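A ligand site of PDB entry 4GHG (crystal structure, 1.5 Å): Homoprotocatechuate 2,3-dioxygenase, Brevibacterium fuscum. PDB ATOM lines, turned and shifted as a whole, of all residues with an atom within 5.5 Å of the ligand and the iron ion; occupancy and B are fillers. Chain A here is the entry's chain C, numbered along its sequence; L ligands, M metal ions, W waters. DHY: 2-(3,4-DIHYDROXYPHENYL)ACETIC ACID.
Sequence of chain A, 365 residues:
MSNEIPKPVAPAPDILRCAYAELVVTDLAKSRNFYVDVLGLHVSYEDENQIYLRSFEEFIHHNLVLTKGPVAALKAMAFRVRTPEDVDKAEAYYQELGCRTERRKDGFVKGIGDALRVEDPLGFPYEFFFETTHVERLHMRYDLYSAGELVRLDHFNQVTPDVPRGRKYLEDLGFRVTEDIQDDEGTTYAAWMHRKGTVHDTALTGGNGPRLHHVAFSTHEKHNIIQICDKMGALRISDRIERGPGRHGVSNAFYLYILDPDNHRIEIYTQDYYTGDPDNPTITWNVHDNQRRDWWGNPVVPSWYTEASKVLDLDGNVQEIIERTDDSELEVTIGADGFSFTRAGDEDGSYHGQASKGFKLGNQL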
ATOM      1  N   HIS A 155     -13.880  -1.914 -14.153  1.00  0.00           N
ATOM      2  CA  HIS A 155     -12.446  -2.031 -14.419  1.00  0.00           C
ATOM      3  C   HIS A 155     -11.615  -1.581 -13.249  1.00  0.00           C
ATOM      4  O   HIS A 155     -12.141  -1.004 -12.284  1.00  0.00           O
ATOM      5  CB  HIS A 155     -12.043  -1.245 -15.685  1.00  0.00           C
ATOM      6  CG  HIS A 155     -12.234   0.247 -15.579  1.00  0.00           C
ATOM      7  ND1 HIS A 155     -13.355   0.862 -16.008  1.00  0.00           N
ATOM      8  CD2 HIS A 155     -11.372   1.233 -15.129  1.00  0.00           C
ATOM      9  CE1 HIS A 155     -13.232   2.190 -15.824  1.00  0.00           C
ATOM     10  NE2 HIS A 155     -12.020   2.433 -15.271  1.00  0.00           N
ATOM     11  N   ASN A 157      -7.597   0.470 -12.666  1.00  0.00           N
ATOM     12  CA  ASN A 157      -6.586   1.265 -13.314  1.00  0.00           C
ATOM     13  C   ASN A 157      -5.359   1.264 -12.394  1.00  0.00           C
ATOM     14  O   ASN A 157      -5.476   1.550 -11.203  1.00  0.00           O
ATOM     15  CB  ASN A 157      -7.069   2.676 -13.634  1.00  0.00           C
ATOM     16  CG  ASN A 157      -6.043   3.499 -14.381  1.00  0.00           C
ATOM     17  OD1 ASN A 157      -4.921   3.737 -13.893  1.00  0.00           O
ATOM     18  ND2 ASN A 157      -6.424   3.968 -15.569  1.00  0.00           N
ATOM     19  N   TRP A 192      -5.277   1.322 -22.289  1.00  0.00           N
ATOM     20  CA  TRP A 192      -6.499   0.671 -21.799  1.00  0.00           C
ATOM     21  C   TRP A 192      -6.626  -0.653 -22.492  1.00  0.00           C
ATOM     22  O   TRP A 192      -6.382  -0.735 -23.699  1.00  0.00           O
ATOM     23  CB  TRP A 192      -7.723   1.532 -22.171  1.00  0.00           C
ATOM     24  CG  TRP A 192      -7.849   2.792 -21.342  1.00  0.00           C
ATOM     25  CD1 TRP A 192      -8.754   3.010 -20.328  1.00  0.00           C
ATOM     26  CD2 TRP A 192      -7.070   4.027 -21.438  1.00  0.00           C
ATOM     27  NE1 TRP A 192      -8.591   4.264 -19.781  1.00  0.00           N
ATOM     28  CE2 TRP A 192      -7.587   4.928 -20.406  1.00  0.00           C
ATOM     29  CE3 TRP A 192      -6.032   4.480 -22.252  1.00  0.00           C
ATOM     30  CZ2 TRP A 192      -7.080   6.217 -20.221  1.00  0.00           C
ATOM     31  CZ3 TRP A 192      -5.519   5.768 -22.048  1.00  0.00           C
ATOM     32  CH2 TRP A 192      -6.028   6.613 -21.066  1.00  0.00           C
ATOM     33  N   HIS A 200     -12.256  -1.592 -21.314  1.00  0.00           N
ATOM     34  CA  HIS A 200     -11.184  -2.160 -20.492  1.00  0.00           C
ATOM     35  C   HIS A 200     -11.669  -2.981 -19.318  1.00  0.00           C
ATOM     36  O   HIS A 200     -12.760  -2.784 -18.803  1.00  0.00           O
ATOM     37  CB  HIS A 200     -10.209  -1.082 -19.989  1.00  0.00           C
ATOM     38  CG  HIS A 200     -10.836   0.139 -19.307  1.00  0.00           C
ATOM     39  ND1 HIS A 200     -12.046   0.609 -19.621  1.00  0.00           N
ATOM     40  CD2 HIS A 200     -10.318   1.013 -18.353  1.00  0.00           C
ATOM     41  CE1 HIS A 200     -12.287   1.736 -18.912  1.00  0.00           C
ATOM     42  NE2 HIS A 200     -11.229   1.991 -18.177  1.00  0.00           N
ATOM     43  N   HIS A 214      -7.414   3.528  -9.447  1.00  0.00           N
ATOM     44  CA  HIS A 214      -8.834   3.470  -9.041  1.00  0.00           C
ATOM     45  C   HIS A 214      -9.474   2.151  -9.330  1.00  0.00           C
ATOM     46  O   HIS A 214      -8.930   1.325 -10.067  1.00  0.00           O
ATOM     47  CB  HIS A 214      -9.656   4.596  -9.691  1.00  0.00           C
ATOM     48  CG  HIS A 214      -9.638   4.627 -11.203  1.00  0.00           C
ATOM     49  ND1 HIS A 214      -8.762   5.366 -11.894  1.00  0.00           N
ATOM     50  CD2 HIS A 214     -10.493   4.057 -12.131  1.00  0.00           C
ATOM     51  CE1 HIS A 214      -9.009   5.255 -13.209  1.00  0.00           C
ATOM     52  NE2 HIS A 214     -10.062   4.453 -13.365  1.00  0.00           N
ATOM     53  N   ALA A 216     -13.366   1.040 -10.751  1.00  0.00           N
ATOM     54  CA  ALA A 216     -14.519   1.681 -11.421  1.00  0.00           C
ATOM     55  C   ALA A 216     -15.750   0.809 -11.424  1.00  0.00           C
ATOM     56  O   ALA A 216     -15.678  -0.398 -11.730  1.00  0.00           O
ATOM     57  CB  ALA A 216     -14.182   2.015 -12.860  1.00  0.00           C
ATOM     58  N   ARG A 243     -12.784  14.836  -9.213  1.00  0.00           N
ATOM     59  CA  ARG A 243     -12.705  15.213 -10.623  1.00  0.00           C
ATOM     60  C   ARG A 243     -13.979  14.762 -11.298  1.00  0.00           C
ATOM     61  O   ARG A 243     -14.448  13.644 -11.089  1.00  0.00           O
ATOM     62  CB  ARG A 243     -11.497  14.568 -11.289  1.00  0.00           C
ATOM     63  CG  ARG A 243     -11.464  14.706 -12.798  1.00  0.00           C
ATOM     64  CD  ARG A 243     -10.171  14.222 -13.460  1.00  0.00           C
ATOM     65  NE  ARG A 243     -10.438  14.213 -14.887  1.00  0.00           N
ATOM     66  CZ  ARG A 243     -10.107  13.261 -15.752  1.00  0.00           C
ATOM     67  NH1 ARG A 243      -9.273  12.276 -15.434  1.00  0.00           N
ATOM     68  NH2 ARG A 243     -10.581  13.317 -16.995  1.00  0.00           N
ATOM     69  N   HIS A 248     -15.476  11.349 -20.919  1.00  0.00           N
ATOM     70  CA  HIS A 248     -14.138  10.995 -21.321  1.00  0.00           C
ATOM     71  C   HIS A 248     -13.959  11.123 -22.818  1.00  0.00           C
ATOM     72  O   HIS A 248     -14.886  10.826 -23.592  1.00  0.00           O
ATOM     73  CB  HIS A 248     -13.815   9.535 -20.992  1.00  0.00           C
ATOM     74  CG  HIS A 248     -13.547   9.237 -19.538  1.00  0.00           C
ATOM     75  ND1 HIS A 248     -12.608   9.890 -18.802  1.00  0.00           N
ATOM     76  CD2 HIS A 248     -14.058   8.232 -18.709  1.00  0.00           C
ATOM     77  CE1 HIS A 248     -12.541   9.345 -17.575  1.00  0.00           C
ATOM     78  NE2 HIS A 248     -13.441   8.344 -17.513  1.00  0.00           N
ATOM     79  N   GLY A 249     -12.748  11.468 -23.223  1.00  0.00           N
ATOM     80  CA  GLY A 249     -12.349  11.325 -24.629  1.00  0.00           C
ATOM     81  C   GLY A 249     -12.059   9.843 -24.874  1.00  0.00           C
ATOM     82  O   GLY A 249     -12.875   9.148 -25.486  1.00  0.00           O
ATOM     83  N   VAL A 250     -10.922   9.366 -24.365  1.00  0.00           N
ATOM     84  CA  VAL A 250     -10.643   7.925 -24.296  1.00  0.00           C
ATOM     85  C   VAL A 250     -11.823   7.228 -23.601  1.00  0.00           C
ATOM     86  O   VAL A 250     -12.231   7.606 -22.503  1.00  0.00           O
ATOM     87  CB  VAL A 250      -9.367   7.648 -23.458  1.00  0.00           C
ATOM     88  CG1 VAL A 250      -9.167   6.156 -23.205  1.00  0.00           C
ATOM     89  CG2 VAL A 250      -8.145   8.268 -24.121  1.00  0.00           C
ATOM     90  N   SER A 251     -12.355   6.211 -24.254  1.00  0.00           N
ATOM     91  CA  SER A 251     -13.510   5.403 -23.822  1.00  0.00           C
ATOM     92  C   SER A 251     -14.873   5.968 -24.138  1.00  0.00           C
ATOM     93  O   SER A 251     -15.826   5.177 -24.211  1.00  0.00           O
ATOM     94  CB  SER A 251     -13.480   5.020 -22.345  1.00  0.00           C
ATOM     95  OG  SER A 251     -14.000   6.050 -21.514  1.00  0.00           O
ATOM     96  N   TYR A 255     -18.346   9.986 -16.661  1.00  0.00           N
ATOM     97  CA  TYR A 255     -17.519   9.576 -15.518  1.00  0.00           C
ATOM     98  C   TYR A 255     -17.556  10.559 -14.361  1.00  0.00           C
ATOM     99  O   TYR A 255     -17.927  11.732 -14.506  1.00  0.00           O
ATOM    100  CB  TYR A 255     -16.069   9.419 -15.963  1.00  0.00           C
ATOM    101  CG  TYR A 255     -15.327  10.727 -16.199  1.00  0.00           C
ATOM    102  CD1 TYR A 255     -15.327  11.336 -17.445  1.00  0.00           C
ATOM    103  CD2 TYR A 255     -14.671  11.385 -15.163  1.00  0.00           C
ATOM    104  CE1 TYR A 255     -14.654  12.549 -17.654  1.00  0.00           C
ATOM    105  CE2 TYR A 255     -14.024  12.590 -15.363  1.00  0.00           C
ATOM    106  CZ  TYR A 255     -14.022  13.163 -16.612  1.00  0.00           C
ATOM    107  OH  TYR A 255     -13.379  14.349 -16.792  1.00  0.00           O
ATOM    108  N   TYR A 257     -14.936  10.870 -10.501  1.00  0.00           N
ATOM    109  CA  TYR A 257     -13.986  10.292  -9.542  1.00  0.00           C
ATOM    110  C   TYR A 257     -14.203  10.860  -8.155  1.00  0.00           C
ATOM    111  O   TYR A 257     -14.264  12.083  -7.968  1.00  0.00           O
ATOM    112  CB  TYR A 257     -12.538  10.564  -9.951  1.00  0.00           C
ATOM    113  CG  TYR A 257     -12.166  10.009 -11.275  1.00  0.00           C
ATOM    114  CD1 TYR A 257     -11.671   8.701 -11.418  1.00  0.00           C
ATOM    115  CD2 TYR A 257     -12.245  10.800 -12.404  1.00  0.00           C
ATOM    116  CE1 TYR A 257     -11.327   8.193 -12.665  1.00  0.00           C
ATOM    117  CE2 TYR A 257     -11.867  10.308 -13.650  1.00  0.00           C
ATOM    118  CZ  TYR A 257     -11.409   9.023 -13.768  1.00  0.00           C
ATOM    119  OH  TYR A 257     -11.071   8.610 -15.015  1.00  0.00           O
ATOM    120  N   GLU A 267     -14.005   5.365  -9.414  1.00  0.00           N
ATOM    121  CA  GLU A 267     -14.615   5.973 -10.584  1.00  0.00           C
ATOM    122  C   GLU A 267     -16.023   5.433 -10.753  1.00  0.00           C
ATOM    123  O   GLU A 267     -16.259   4.233 -10.547  1.00  0.00           O
ATOM    124  CB  GLU A 267     -13.811   5.657 -11.858  1.00  0.00           C
ATOM    125  CG  GLU A 267     -14.309   6.392 -13.090  1.00  0.00           C
ATOM    126  CD  GLU A 267     -13.555   6.037 -14.339  1.00  0.00           C
ATOM    127  OE1 GLU A 267     -12.712   5.121 -14.285  1.00  0.00           O
ATOM    128  OE2 GLU A 267     -13.793   6.662 -15.373  1.00  0.00           O
ATOM    129  N   TYR A 269     -18.865   5.281 -13.863  1.00  0.00           N
ATOM    130  CA  TYR A 269     -18.599   5.197 -15.292  1.00  0.00           C
ATOM    131  C   TYR A 269     -19.847   4.683 -15.992  1.00  0.00           C
ATOM    132  O   TYR A 269     -20.533   3.808 -15.486  1.00  0.00           O
ATOM    133  CB  TYR A 269     -17.472   4.172 -15.441  1.00  0.00           C
ATOM    134  CG  TYR A 269     -16.867   3.864 -16.794  1.00  0.00           C
ATOM    135  CD1 TYR A 269     -15.729   4.531 -17.243  1.00  0.00           C
ATOM    136  CD2 TYR A 269     -17.354   2.820 -17.571  1.00  0.00           C
ATOM    137  CE1 TYR A 269     -15.100   4.171 -18.428  1.00  0.00           C
ATOM    138  CE2 TYR A 269     -16.731   2.474 -18.763  1.00  0.00           C
ATOM    139  CZ  TYR A 269     -15.614   3.155 -19.193  1.00  0.00           C
ATOM    140  OH  TYR A 269     -15.003   2.782 -20.373  1.00  0.00           O
ATOM    141  N   ARG A 292      -8.679  14.661 -24.731  1.00  0.00           N
ATOM    142  CA  ARG A 292      -8.396  13.212 -24.610  1.00  0.00           C
ATOM    143  C   ARG A 292      -8.901  12.588 -23.317  1.00  0.00           C
ATOM    144  O   ARG A 292      -9.265  11.416 -23.287  1.00  0.00           O
ATOM    145  CB  ARG A 292      -6.892  12.976 -24.773  1.00  0.00           C
ATOM    146  CG  ARG A 292      -6.093  13.293 -23.517  1.00  0.00           C
ATOM    147  CD  ARG A 292      -4.609  13.442 -23.715  1.00  0.00           C
ATOM    148  NE  ARG A 292      -4.015  13.751 -22.409  1.00  0.00           N
ATOM    149  CZ  ARG A 292      -4.083  14.941 -21.820  1.00  0.00           C
ATOM    150  NH1 ARG A 292      -4.668  15.976 -22.422  1.00  0.00           N
ATOM    151  NH2 ARG A 292      -3.548  15.099 -20.622  1.00  0.00           N
ATOM    152  N   ARG A 293      -8.852  13.355 -22.239  1.00  0.00           N
ATOM    153  CA  ARG A 293      -9.242  12.862 -20.943  1.00  0.00           C
ATOM    154  C   ARG A 293     -10.640  13.346 -20.606  1.00  0.00           C
ATOM    155  O   ARG A 293     -11.563  12.559 -20.487  1.00  0.00           O
ATOM    156  CB  ARG A 293      -8.185  13.233 -19.890  1.00  0.00           C
ATOM    157  CG  ARG A 293      -6.935  12.325 -20.030  1.00  0.00           C
ATOM    158  CD  ARG A 293      -6.106  12.270 -18.763  1.00  0.00           C
ATOM    159  NE  ARG A 293      -4.955  11.373 -18.889  1.00  0.00           N
ATOM    160  CZ  ARG A 293      -4.955  10.069 -18.646  1.00  0.00           C
ATOM    161  NH1 ARG A 293      -6.035   9.424 -18.238  1.00  0.00           N
ATOM    162  NH2 ARG A 293      -3.854   9.379 -18.802  1.00  0.00           N
ATOM    163  N   ASP A 294     -10.806  14.662 -20.513  1.00  0.00           N
ATOM    164  CA  ASP A 294     -12.128  15.244 -20.470  1.00  0.00           C
ATOM    165  C   ASP A 294     -12.440  15.814 -21.854  1.00  0.00           C
ATOM    166  O   ASP A 294     -11.761  16.716 -22.357  1.00  0.00           O
ATOM    167  CB  ASP A 294     -12.253  16.311 -19.413  1.00  0.00           C
ATOM    168  CG  ASP A 294     -13.680  16.737 -19.219  1.00  0.00           C
ATOM    169  OD1 ASP A 294     -14.421  16.019 -18.499  1.00  0.00           O
ATOM    170  OD2 ASP A 294     -14.071  17.785 -19.782  1.00  0.00           O
ATOM    171  N   TRP A 304      -5.045  14.007  -9.469  1.00  0.00           N
ATOM    172  CA  TRP A 304      -5.456  12.838 -10.272  1.00  0.00           C
ATOM    173  C   TRP A 304      -4.249  12.145 -10.869  1.00  0.00           C
ATOM    174  O   TRP A 304      -4.205  10.921 -10.943  1.00  0.00           O
ATOM    175  CB  TRP A 304      -6.448  13.255 -11.346  1.00  0.00           C
ATOM    176  CG  TRP A 304      -7.196  12.100 -11.935  1.00  0.00           C
ATOM    177  CD1 TRP A 304      -8.390  11.567 -11.488  1.00  0.00           C
ATOM    178  CD2 TRP A 304      -6.783  11.260 -13.042  1.00  0.00           C
ATOM    179  NE1 TRP A 304      -8.756  10.505 -12.245  1.00  0.00           N
ATOM    180  CE2 TRP A 304      -7.837  10.261 -13.214  1.00  0.00           C
ATOM    181  CE3 TRP A 304      -5.681  11.226 -13.897  1.00  0.00           C
ATOM    182  CZ2 TRP A 304      -7.778   9.275 -14.188  1.00  0.00           C
ATOM    183  CZ3 TRP A 304      -5.627  10.231 -14.870  1.00  0.00           C
ATOM    184  CH2 TRP A 304      -6.655   9.279 -15.015  1.00  0.00           C
HETATM  185  C1  DHY L   1      -9.940   7.955 -19.003  1.00  0.00           C
HETATM  186  C2  DHY L   1      -9.672   7.613 -17.638  1.00  0.00           C
HETATM  187  C3  DHY L   1     -10.389   6.559 -17.039  1.00  0.00           C
HETATM  188  C4  DHY L   1     -11.321   5.802 -17.849  1.00  0.00           C
HETATM  189  C5  DHY L   1     -11.419   6.014 -19.242  1.00  0.00           C
HETATM  190  C6  DHY L   1     -10.787   7.162 -19.825  1.00  0.00           C
HETATM  191  C7  DHY L   1      -9.259   9.196 -19.542  1.00  0.00           C
HETATM  192  C8  DHY L   1      -9.483  10.347 -18.518  1.00  0.00           C
HETATM  193  O1  DHY L   1     -10.440  11.103 -18.620  1.00  0.00           O
HETATM  194  O2  DHY L   1      -8.706  10.503 -17.693  1.00  0.00           O
HETATM  195  O3  DHY L   1     -10.258   6.264 -15.717  1.00  0.00           O
HETATM  196  O4  DHY L   1     -12.006   4.781 -17.216  1.00  0.00           O
HETATM  197 FE    FE M   1     -11.098   4.415 -15.258  1.00  0.00          FE
HETATM  198  O   HOH W   1      -9.225   3.417 -16.442  1.00  0.00           O
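Merely in contact with the iron ion: His 200. Of the 19 residues printed, 4 come within 4 Å of the iron ion. Along chain A the residues within 4 Å of the iron ion span positions 155 to 267.
A ring nitrogen (ND1) of His 248 lies within hydrogen-bond range of an oxygen (O1) of the ligand, 2.5 Å away. An oxygen (O3) of the ligand lies close to the side-chain hydroxyl (OH) of Tyr 257, 2.6 Å away. O of Arg 293 sits close to O1 of the ligand (2.6 Å). The guanidinium group (NH1) of Arg 293 is in salt-bridge range of an oxygen (O2) of the ligand (2.9 Å). The guanidinium group of Arg 243 lies within salt-bridge range of an oxygen (O1) of the ligand, 2.7 Å away. An oxygen (O4) of the ligand lies close to a ring nitrogen (NE2) of His 200 (3.1 Å).
Water W1 lies within hydrogen-bond range of ND2 of Asn 157 (3.0 Å) and NE2 of His 200 (3.0 Å).
The iron ion is bound by the side-chain carboxylate (OE1) of Glu 267, an oxygen (O3) of the ligand, a ring nitrogen (NE2) of His 214, a ring nitrogen (NE2) of His 155, an oxygen (O4) of the ligand and water W1.
A ring nitrogen (NE2) of His 248 is in hydrogen-bond range of the side-chain carboxylate of Glu 267 (2.7 Å). OH of Tyr 257 sits at hydrogen-bond distance from OE2 of Glu 267. ND1 of His 155 sits close to NE2 of His 200, 3.2 Å away. N of Ala 216 is in hydrogen-bond range of O of His 155. A ring nitrogen (ND1) of His 248 sits close to the backbone carbonyl oxygen (O) of Arg 293 (3.3 Å). N of Tyr 257 sits at hydrogen-bond distance from O of Arg 243 (2.9 Å). The backbone carbonyl oxygen (O) of Arg 293 is in hydrogen-bond range of the backbone NH (N) of Gly 249. NH2 of Arg 243 is in hydrogen-bond range of OH of Tyr 255, at 3.0 Å.
Residues that only touch the ligand: Val 250 (3.1 Å), Trp 192 (3.4 Å), Tyr 269 (3.4 Å), Ser 251 (3.4 Å) and Trp 304 (3.6 Å). Of the 19 residues printed, 13 come within 4 Å of the ligand. The nearest printed residue that does not touch the ligand is Asp 294 (4.05 Å).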
